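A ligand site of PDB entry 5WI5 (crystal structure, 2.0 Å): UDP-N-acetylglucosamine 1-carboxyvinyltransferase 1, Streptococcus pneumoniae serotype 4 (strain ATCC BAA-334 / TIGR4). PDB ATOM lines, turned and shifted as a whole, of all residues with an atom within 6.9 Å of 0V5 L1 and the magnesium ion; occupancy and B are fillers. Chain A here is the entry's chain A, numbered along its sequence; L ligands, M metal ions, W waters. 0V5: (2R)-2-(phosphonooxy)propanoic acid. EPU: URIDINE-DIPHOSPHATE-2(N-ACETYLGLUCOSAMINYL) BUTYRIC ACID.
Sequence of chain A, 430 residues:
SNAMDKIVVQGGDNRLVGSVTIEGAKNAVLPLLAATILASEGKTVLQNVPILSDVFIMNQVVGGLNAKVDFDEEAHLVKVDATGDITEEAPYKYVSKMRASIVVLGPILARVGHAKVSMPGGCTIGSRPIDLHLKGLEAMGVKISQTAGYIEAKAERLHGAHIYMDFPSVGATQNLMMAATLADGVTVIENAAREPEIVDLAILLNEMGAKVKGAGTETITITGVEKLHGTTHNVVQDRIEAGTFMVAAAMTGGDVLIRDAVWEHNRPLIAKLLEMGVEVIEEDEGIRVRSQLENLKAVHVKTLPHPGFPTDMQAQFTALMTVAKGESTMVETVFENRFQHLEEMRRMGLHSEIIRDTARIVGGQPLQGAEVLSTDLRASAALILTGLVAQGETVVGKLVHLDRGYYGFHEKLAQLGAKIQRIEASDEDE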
ATOM      1  N   ASP A  54     -22.514   6.504   2.148  1.00  0.00           N
ATOM      2  CA  ASP A  54     -23.351   6.398   3.356  1.00  0.00           C
ATOM      3  C   ASP A  54     -24.354   5.263   3.254  1.00  0.00           C
ATOM      4  O   ASP A  54     -24.690   4.668   4.276  1.00  0.00           O
ATOM      5  CB  ASP A  54     -24.083   7.735   3.680  1.00  0.00           C
ATOM      6  CG  ASP A  54     -23.166   8.776   4.397  1.00  0.00           C
ATOM      7  OD1 ASP A  54     -21.950   8.578   4.496  1.00  0.00           O
ATOM      8  OD2 ASP A  54     -23.705   9.797   4.863  1.00  0.00           O
ATOM      9  N   TYR A  94     -18.493   0.997  12.212  1.00  0.00           N
ATOM     10  CA  TYR A  94     -19.431   1.716  11.333  1.00  0.00           C
ATOM     11  C   TYR A  94     -19.853   3.062  11.898  1.00  0.00           C
ATOM     12  O   TYR A  94     -19.825   4.075  11.201  1.00  0.00           O
ATOM     13  CB  TYR A  94     -20.691   0.868  11.001  1.00  0.00           C
ATOM     14  CG  TYR A  94     -20.369  -0.510  10.465  1.00  0.00           C
ATOM     15  CD1 TYR A  94     -19.429  -0.679   9.445  1.00  0.00           C
ATOM     16  CD2 TYR A  94     -21.036  -1.627  10.920  1.00  0.00           C
ATOM     17  CE1 TYR A  94     -19.133  -1.941   8.948  1.00  0.00           C
ATOM     18  CE2 TYR A  94     -20.768  -2.887  10.406  1.00  0.00           C
ATOM     19  CZ  TYR A  94     -19.818  -3.045   9.438  1.00  0.00           C
ATOM     20  OH  TYR A  94     -19.562  -4.299   8.956  1.00  0.00           O
ATOM     21  N   VAL A  95     -20.224   3.095  13.171  1.00  0.00           N
ATOM     22  CA  VAL A  95     -20.667   4.348  13.787  1.00  0.00           C
ATOM     23  C   VAL A  95     -19.567   5.418  13.755  1.00  0.00           C
ATOM     24  O   VAL A  95     -19.866   6.622  13.576  1.00  0.00           O
ATOM     25  CB  VAL A  95     -21.117   4.130  15.222  1.00  0.00           C
ATOM     26  CG1 VAL A  95     -21.598   5.455  15.849  1.00  0.00           C
ATOM     27  CG2 VAL A  95     -22.227   3.079  15.285  1.00  0.00           C
ATOM     28  N   SER A  96     -18.315   5.008  13.929  1.00  0.00           N
ATOM     29  CA  SER A  96     -17.204   5.953  13.890  1.00  0.00           C
ATOM     30  C   SER A  96     -17.002   6.580  12.503  1.00  0.00           C
ATOM     31  O   SER A  96     -16.426   7.634  12.405  1.00  0.00           O
ATOM     32  CB  SER A  96     -15.897   5.294  14.365  1.00  0.00           C
ATOM     33  OG  SER A  96     -15.499   4.276  13.466  1.00  0.00           O
ATOM     34  N   LYS A  97     -17.487   5.949  11.455  1.00  0.00           N
ATOM     35  CA  LYS A  97     -17.378   6.504  10.081  1.00  0.00           C
ATOM     36  C   LYS A  97     -18.670   7.239   9.656  1.00  0.00           C
ATOM     37  O   LYS A  97     -18.678   7.975   8.664  1.00  0.00           O
ATOM     38  CB  LYS A  97     -17.085   5.404   9.073  1.00  0.00           C
ATOM     39  CG  LYS A  97     -15.734   4.740   9.233  1.00  0.00           C
ATOM     40  CD  LYS A  97     -15.638   3.383   8.510  1.00  0.00           C
ATOM     41  CE  LYS A  97     -15.083   3.364   7.093  1.00  0.00           C
ATOM     42  NZ  LYS A  97     -15.951   3.986   6.063  1.00  0.00           N
ATOM     43  N   MET A  98     -19.747   7.048  10.412  1.00  0.00           N
ATOM     44  CA  MET A  98     -21.021   7.653  10.072  1.00  0.00           C
ATOM     45  C   MET A  98     -21.951   7.634  11.291  1.00  0.00           C
ATOM     46  O   MET A  98     -22.663   6.657  11.524  1.00  0.00           O
ATOM     47  CB  MET A  98     -21.649   6.906   8.880  1.00  0.00           C
ATOM     48  CG  MET A  98     -22.936   7.497   8.393  1.00  0.00           C
ATOM     49  SD  MET A  98     -23.628   6.568   7.030  1.00  0.00           S
ATOM     50  CE  MET A  98     -24.527   5.274   7.864  1.00  0.00           C
ATOM     51  N   ARG A  99     -21.961   8.734  12.021  1.00  0.00           N
ATOM     52  CA  ARG A  99     -22.771   8.820  13.245  1.00  0.00           C
ATOM     53  C   ARG A  99     -24.285   8.602  13.010  1.00  0.00           C
ATOM     54  O   ARG A  99     -25.001   8.254  13.940  1.00  0.00           O
ATOM     55  CB  ARG A  99     -22.521  10.115  13.996  1.00  0.00           C
ATOM     56  CG  ARG A  99     -23.023  11.334  13.281  1.00  0.00           C
ATOM     57  CD  ARG A  99     -22.473  12.634  13.899  1.00  0.00           C
ATOM     58  NE  ARG A  99     -22.683  12.826  15.329  1.00  0.00           N
ATOM     59  CZ  ARG A  99     -21.738  12.797  16.291  1.00  0.00           C
ATOM     60  NH1 ARG A  99     -22.100  13.017  17.569  1.00  0.00           N
ATOM     61  NH2 ARG A  99     -20.466  12.606  15.996  1.00  0.00           N
ATOM     62  N   ALA A 100     -24.731   8.752  11.785  1.00  0.00           N
ATOM     63  CA  ALA A 100     -26.150   8.499  11.430  1.00  0.00           C
ATOM     64  C   ALA A 100     -26.519   7.043  11.626  1.00  0.00           C
ATOM     65  O   ALA A 100     -27.703   6.695  11.643  1.00  0.00           O
ATOM     66  CB  ALA A 100     -26.431   8.919   9.999  1.00  0.00           C
ATOM     67  N   PRO A 120     -21.567   7.789  19.418  1.00  0.00           N
ATOM     68  CA  PRO A 120     -20.822   8.628  18.487  1.00  0.00           C
ATOM     69  C   PRO A 120     -19.875   9.559  19.222  1.00  0.00           C
ATOM     70  O   PRO A 120     -20.207  10.073  20.274  1.00  0.00           O
ATOM     71  CB  PRO A 120     -21.916   9.461  17.779  1.00  0.00           C
ATOM     72  CG  PRO A 120     -23.134   8.574  17.884  1.00  0.00           C
ATOM     73  CD  PRO A 120     -23.019   7.949  19.246  1.00  0.00           C
ATOM     74  N   GLY A 122     -16.711  12.585  18.085  1.00  0.00           N
ATOM     75  CA  GLY A 122     -16.626  13.930  17.538  1.00  0.00           C
ATOM     76  C   GLY A 122     -16.930  14.047  16.067  1.00  0.00           C
ATOM     77  O   GLY A 122     -16.695  13.114  15.272  1.00  0.00           O
ATOM     78  N   CYS A 123     -17.509  15.187  15.712  1.00  0.00           N
ATOM     79  CA  CYS A 123     -17.816  15.523  14.336  1.00  0.00           C
ATOM     80  C   CYS A 123     -17.470  17.011  14.213  1.00  0.00           C
ATOM     81  O   CYS A 123     -17.834  17.805  15.081  1.00  0.00           O
ATOM     82  CB  CYS A 123     -19.298  15.247  14.009  1.00  0.00           C
ATOM     83  SG  CYS A 123     -19.792  15.712  12.311  1.00  0.00           S
ATOM     84  N   THR A 124     -16.796  17.369  13.120  1.00  0.00           N
ATOM     85  CA  THR A 124     -16.309  18.738  12.884  1.00  0.00           C
ATOM     86  C   THR A 124     -17.380  19.804  12.705  1.00  0.00           C
ATOM     87  O   THR A 124     -17.118  20.952  13.045  1.00  0.00           O
ATOM     88  CB  THR A 124     -15.376  18.804  11.640  1.00  0.00           C
ATOM     89  OG1 THR A 124     -16.090  18.411  10.475  1.00  0.00           O
ATOM     90  CG2 THR A 124     -14.206  17.840  11.766  1.00  0.00           C
ATOM     91  N   ILE A 125     -18.559  19.465  12.208  1.00  0.00           N
ATOM     92  CA  ILE A 125     -19.554  20.530  11.921  1.00  0.00           C
ATOM     93  C   ILE A 125     -20.285  21.059  13.159  1.00  0.00           C
ATOM     94  O   ILE A 125     -21.027  22.051  13.078  1.00  0.00           O
ATOM     95  CB  ILE A 125     -20.562  20.178  10.802  1.00  0.00           C
ATOM     96  CG1 ILE A 125     -21.545  19.079  11.199  1.00  0.00           C
ATOM     97  CG2 ILE A 125     -19.814  19.791   9.503  1.00  0.00           C
ATOM     98  CD1 ILE A 125     -22.711  18.990  10.238  1.00  0.00           C
ATOM     99  N   GLY A 126     -20.087  20.396  14.289  1.00  0.00           N
ATOM    100  CA  GLY A 126     -20.750  20.829  15.532  1.00  0.00           C
ATOM    101  C   GLY A 126     -20.715  19.791  16.628  1.00  0.00           C
ATOM    102  O   GLY A 126     -20.341  18.650  16.425  1.00  0.00           O
ATOM    103  N   ARG A 128     -23.214  18.076  18.237  1.00  0.00           N
ATOM    104  CA  ARG A 128     -24.002  16.815  17.927  1.00  0.00           C
ATOM    105  C   ARG A 128     -24.271  15.772  19.018  1.00  0.00           C
ATOM    106  O   ARG A 128     -24.088  14.566  18.819  1.00  0.00           O
ATOM    107  CB  ARG A 128     -23.540  16.096  16.615  1.00  0.00           C
ATOM    108  CG  ARG A 128     -23.367  17.107  15.492  1.00  0.00           C
ATOM    109  CD  ARG A 128     -23.080  16.478  14.184  1.00  0.00           C
ATOM    110  NE  ARG A 128     -24.261  15.911  13.572  1.00  0.00           N
ATOM    111  CZ  ARG A 128     -24.305  15.440  12.333  1.00  0.00           C
ATOM    112  NH1 ARG A 128     -23.198  15.398  11.596  1.00  0.00           N
ATOM    113  NH2 ARG A 128     -25.460  14.981  11.833  1.00  0.00           N
ATOM    114  N   THR A 375     -14.333  19.870   3.327  1.00  0.00           N
ATOM    115  CA  THR A 375     -14.351  19.655   4.781  1.00  0.00           C
ATOM    116  C   THR A 375     -15.522  18.769   5.225  1.00  0.00           C
ATOM    117  O   THR A 375     -15.452  18.124   6.271  1.00  0.00           O
ATOM    118  CB  THR A 375     -14.444  20.999   5.514  1.00  0.00           C
ATOM    119  OG1 THR A 375     -15.480  21.794   4.935  1.00  0.00           O
ATOM    120  CG2 THR A 375     -13.130  21.757   5.348  1.00  0.00           C
ATOM    121  N   ASP A 376     -16.577  18.738   4.418  1.00  0.00           N
ATOM    122  CA  ASP A 376     -17.760  17.951   4.703  1.00  0.00           C
ATOM    123  C   ASP A 376     -18.589  17.858   3.430  1.00  0.00           C
ATOM    124  O   ASP A 376     -18.293  18.522   2.457  1.00  0.00           O
ATOM    125  CB  ASP A 376     -18.573  18.603   5.838  1.00  0.00           C
ATOM    126  CG  ASP A 376     -18.939  20.027   5.545  1.00  0.00           C
ATOM    127  OD1 ASP A 376     -19.977  20.243   4.855  1.00  0.00           O
ATOM    128  OD2 ASP A 376     -18.227  20.945   6.039  1.00  0.00           O
ATOM    129  N   LEU A 377     -19.631  17.030   3.458  1.00  0.00           N
ATOM    130  CA  LEU A 377     -20.459  16.773   2.269  1.00  0.00           C
ATOM    131  C   LEU A 377     -20.967  18.017   1.510  1.00  0.00           C
ATOM    132  O   LEU A 377     -20.652  18.196   0.330  1.00  0.00           O
ATOM    133  CB  LEU A 377     -21.640  15.887   2.697  1.00  0.00           C
ATOM    134  CG  LEU A 377     -22.742  15.652   1.672  1.00  0.00           C
ATOM    135  CD1 LEU A 377     -22.199  15.128   0.353  1.00  0.00           C
ATOM    136  CD2 LEU A 377     -23.779  14.688   2.245  1.00  0.00           C
ATOM    137  N   HIS A 401     -15.739  13.131   1.150  1.00  0.00           N
ATOM    138  CA  HIS A 401     -16.916  13.836   1.686  1.00  0.00           C
ATOM    139  C   HIS A 401     -18.047  13.928   0.653  1.00  0.00           C
ATOM    140  O   HIS A 401     -19.187  13.664   0.975  1.00  0.00           O
ATOM    141  CB  HIS A 401     -16.557  15.241   2.211  1.00  0.00           C
ATOM    142  CG  HIS A 401     -15.548  15.225   3.310  1.00  0.00           C
ATOM    143  ND1 HIS A 401     -15.822  14.694   4.552  1.00  0.00           N
ATOM    144  CD2 HIS A 401     -14.277  15.683   3.365  1.00  0.00           C
ATOM    145  CE1 HIS A 401     -14.747  14.812   5.321  1.00  0.00           C
ATOM    146  NE2 HIS A 401     -13.797  15.408   4.618  1.00  0.00           N
ATOM    147  N   ARG A 404     -20.315  10.885  -0.215  1.00  0.00           N
ATOM    148  CA  ARG A 404     -21.275  10.452   0.790  1.00  0.00           C
ATOM    149  C   ARG A 404     -22.696  10.829   0.405  1.00  0.00           C
ATOM    150  O   ARG A 404     -23.631  10.156   0.813  1.00  0.00           O
ATOM    151  CB  ARG A 404     -20.945  11.054   2.164  1.00  0.00           C
ATOM    152  CG  ARG A 404     -19.649  10.531   2.751  1.00  0.00           C
ATOM    153  CD  ARG A 404     -19.344  11.146   4.082  1.00  0.00           C
ATOM    154  NE  ARG A 404     -20.350  10.798   5.080  1.00  0.00           N
ATOM    155  CZ  ARG A 404     -20.293  11.170   6.347  1.00  0.00           C
ATOM    156  NH1 ARG A 404     -19.285  11.931   6.783  1.00  0.00           N
ATOM    157  NH2 ARG A 404     -21.252  10.804   7.172  1.00  0.00           N
HETATM  158  C1  0V5 L   1     -17.634  14.161  11.141  1.00  0.00           C
HETATM  159  O1  0V5 L   1     -16.863  15.150  11.037  1.00  0.00           O
HETATM  160  O2' 0V5 L   1     -17.191  12.985  11.310  1.00  0.00           O
HETATM  161  C2  0V5 L   1     -19.118  14.478  11.118  1.00  0.00           C
HETATM  162  C3  0V5 L   1     -19.479  15.007   9.726  1.00  0.00           C
HETATM  163  O2  0V5 L   1     -19.976  13.379  11.483  1.00  0.00           O
HETATM  164  P   0V5 L   1     -20.148  12.017  10.610  1.00  0.00           P
HETATM  165  O1P 0V5 L   1     -21.435  12.053   9.845  1.00  0.00           O
HETATM  166  O2P 0V5 L   1     -20.135  10.862  11.592  1.00  0.00           O
HETATM  167  O3P 0V5 L   1     -19.033  11.851   9.596  1.00  0.00           O
HETATM  168  N1U EPU L   2     -29.438  17.914  18.801  1.00  0.00           N
HETATM  169  C2U EPU L   2     -29.304  17.893  20.202  1.00  0.00           C
HETATM  170  N3U EPU L   2     -29.590  16.778  20.864  1.00  0.00           N
HETATM  171  C4U EPU L   2     -30.003  15.658  20.240  1.00  0.00           C
HETATM  172  C5U EPU L   2     -30.132  15.642  18.848  1.00  0.00           C
HETATM  173  C6U EPU L   2     -29.827  16.794  18.149  1.00  0.00           C
HETATM  174  O2U EPU L   2     -28.930  18.896  20.818  1.00  0.00           O
HETATM  175  O4U EPU L   2     -30.253  14.640  20.926  1.00  0.00           O
HETATM  176  C1D EPU L   2     -29.079  19.103  18.055  1.00  0.00           C
HETATM  177  C2D EPU L   2     -27.774  18.741  17.349  1.00  0.00           C
HETATM  178  O2D EPU L   2     -26.572  19.078  18.057  1.00  0.00           O
HETATM  179  C3D EPU L   2     -27.862  19.509  16.076  1.00  0.00           C
HETATM  180  C4D EPU L   2     -29.325  19.826  15.885  1.00  0.00           C
HETATM  181  O4D EPU L   2     -30.051  19.376  17.049  1.00  0.00           O
HETATM  182  O3D EPU L   2     -27.072  20.670  16.195  1.00  0.00           O
HETATM  183  C5D EPU L   2     -29.855  19.140  14.653  1.00  0.00           C
HETATM  184  O5D EPU L   2     -29.540  17.762  14.704  1.00  0.00           O
HETATM  185  PA  EPU L   2     -30.562  16.696  14.150  1.00  0.00           P
HETATM  186  O1A EPU L   2     -30.643  15.587  15.156  1.00  0.00           O
HETATM  187  O2A EPU L   2     -31.825  17.404  13.647  1.00  0.00           O
HETATM  188  O3A EPU L   2     -29.774  16.249  12.815  1.00  0.00           O
HETATM  189  PB  EPU L   2     -29.231  14.762  12.566  1.00  0.00           P
HETATM  190  O1B EPU L   2     -30.380  13.757  12.605  1.00  0.00           O
HETATM  191  O2B EPU L   2     -27.990  14.578  13.363  1.00  0.00           O
HETATM  192  C1  EPU L   2     -29.787  15.005   9.982  1.00  0.00           C
HETATM  193  C2  EPU L   2     -29.061  14.829   8.672  1.00  0.00           C
HETATM  194  C3  EPU L   2     -28.068  15.958   8.506  1.00  0.00           C
HETATM  195  C4  EPU L   2     -28.855  17.271   8.474  1.00  0.00           C
HETATM  196  C5  EPU L   2     -29.569  17.412   9.801  1.00  0.00           C
HETATM  197  C6  EPU L   2     -30.423  18.699   9.967  1.00  0.00           C
HETATM  198  C7  EPU L   2     -29.137  12.428   8.298  1.00  0.00           C
HETATM  199  C8  EPU L   2     -28.392  11.131   8.155  1.00  0.00           C
HETATM  200  N2  EPU L   2     -28.441  13.526   8.573  1.00  0.00           N
HETATM  201  O1  EPU L   2     -28.820  14.918  11.038  1.00  0.00           O
HETATM  202  O3  EPU L   2     -27.416  15.700   7.267  1.00  0.00           O
HETATM  203  O4  EPU L   2     -27.941  18.349   8.323  1.00  0.00           O
HETATM  204  O5  EPU L   2     -30.428  16.296  10.011  1.00  0.00           O
HETATM  205  O6  EPU L   2     -31.329  18.887   8.931  1.00  0.00           O
HETATM  206  O7  EPU L   2     -30.328  12.457   8.137  1.00  0.00           O
HETATM  207  C1E EPU L   2     -25.466  14.419   6.454  1.00  0.00           C
HETATM  208  O1E EPU L   2     -25.991  14.262   5.343  1.00  0.00           O
HETATM  209  O2E EPU L   2     -24.522  13.691   6.866  1.00  0.00           O
HETATM  210  C2E EPU L   2     -25.970  15.571   7.182  1.00  0.00           C
HETATM  211  C3E EPU L   2     -25.141  16.555   7.515  1.00  0.00           C
HETATM  212 MG    MG M   1     -16.922  11.393   9.978  1.00  0.00          MG
HETATM  213  O   HOH W   1     -19.128  11.355  14.018  1.00  0.00           O
HETATM  214  O   HOH W   2     -16.274  12.891   8.554  1.00  0.00           O
HETATM  215  O   HOH W   3     -17.403  10.051  11.411  1.00  0.00           O
HETATM  216  O   HOH W   4     -14.901  11.103  10.523  1.00  0.00           O
HETATM  217  O   HOH W   5     -16.798   9.943   8.559  1.00  0.00           O
HETATM  218  O   HOH W   6     -22.864  14.214   8.991  1.00  0.00           O
HETATM  219  O   HOH W   7     -23.777  10.755   9.801  1.00  0.00           O
HETATM  220  O   HOH W   8     -14.711  14.232  12.278  1.00  0.00           O
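Water W3 lies within hydrogen-bond range of O of Ser 96 (2.8 Å) and O2P of 0V5 L1 (2.9 Å). Water W1 lies within hydrogen-bond range of an oxygen (O2P) of 0V5 L1 (2.7 Å), the guanidinium group (NH2) of Arg 99 (2.7 Å) and the backbone carbonyl oxygen (O) of Gly 122 (3.3 Å). Water W7 lies within hydrogen-bond range of an oxygen (O1P) of 0V5 L1 (2.7 Å) and the backbone NH (N) of Ala 100 (3.0 Å). Water W6 lies within hydrogen-bond range of an oxygen (O1P) of 0V5 L1 (2.7 Å), an oxygen (O2E) of EPU L2 (2.7 Å) and the guanidinium group of Arg 128 (2.9 Å).
The side-chain sulfur (SG) of Cys 123 is in hydrogen-bond range of the guanidinium group (NH1) of Arg 128 (3.5 Å). The side-chain carboxylate (OD1) of Asp 54 lies within salt-bridge range of the guanidinium group (NE) of Arg 404, 2.8 Å away. The backbone carbonyl oxygen of Arg 128 lies within hydrogen-bond range of the guanidinium group of Arg 99, at 2.8 Å.
The magnesium ion is bound by water W3 (2.0 Å), water W5 (2.0 Å), O2' of 0V5 L1 (2.1 Å), water W4 (2.1 Å), water W2 (2.2 Å) and O3P of 0V5 L1 (2.2 Å). The magnesium ion has six donor atoms within binding distance.
Merely in contact with 0V5 L1: Met 98, Arg 128 and Gly 122. Of the 20 residues printed, 7 come within 4 Å of 0V5 L1.
No residue comes within 4 Å of the magnesium ion.
The side-chain sulfur of Cys 123 is covalently linked to a carbon (C2) of 0V5 L1 (1.8 Å). The guanidinium group (NH2) of Arg 404 is in salt-bridge range of an oxygen (O1P) of 0V5 L1, at 3.0 Å. O2P of 0V5 L1 is in hydrogen-bond range of N of Arg 99 (2.8 Å). The backbone NH (N) of Thr 124 is in hydrogen-bond range of an oxygen (O1) of 0V5 L1, 3.0 Å away. OG1 of Thr 124 is in hydrogen-bond range of O1 of 0V5 L1. NH2 of Arg 128 is in salt-bridge range of O2B of EPU L2 (3.0 Å).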
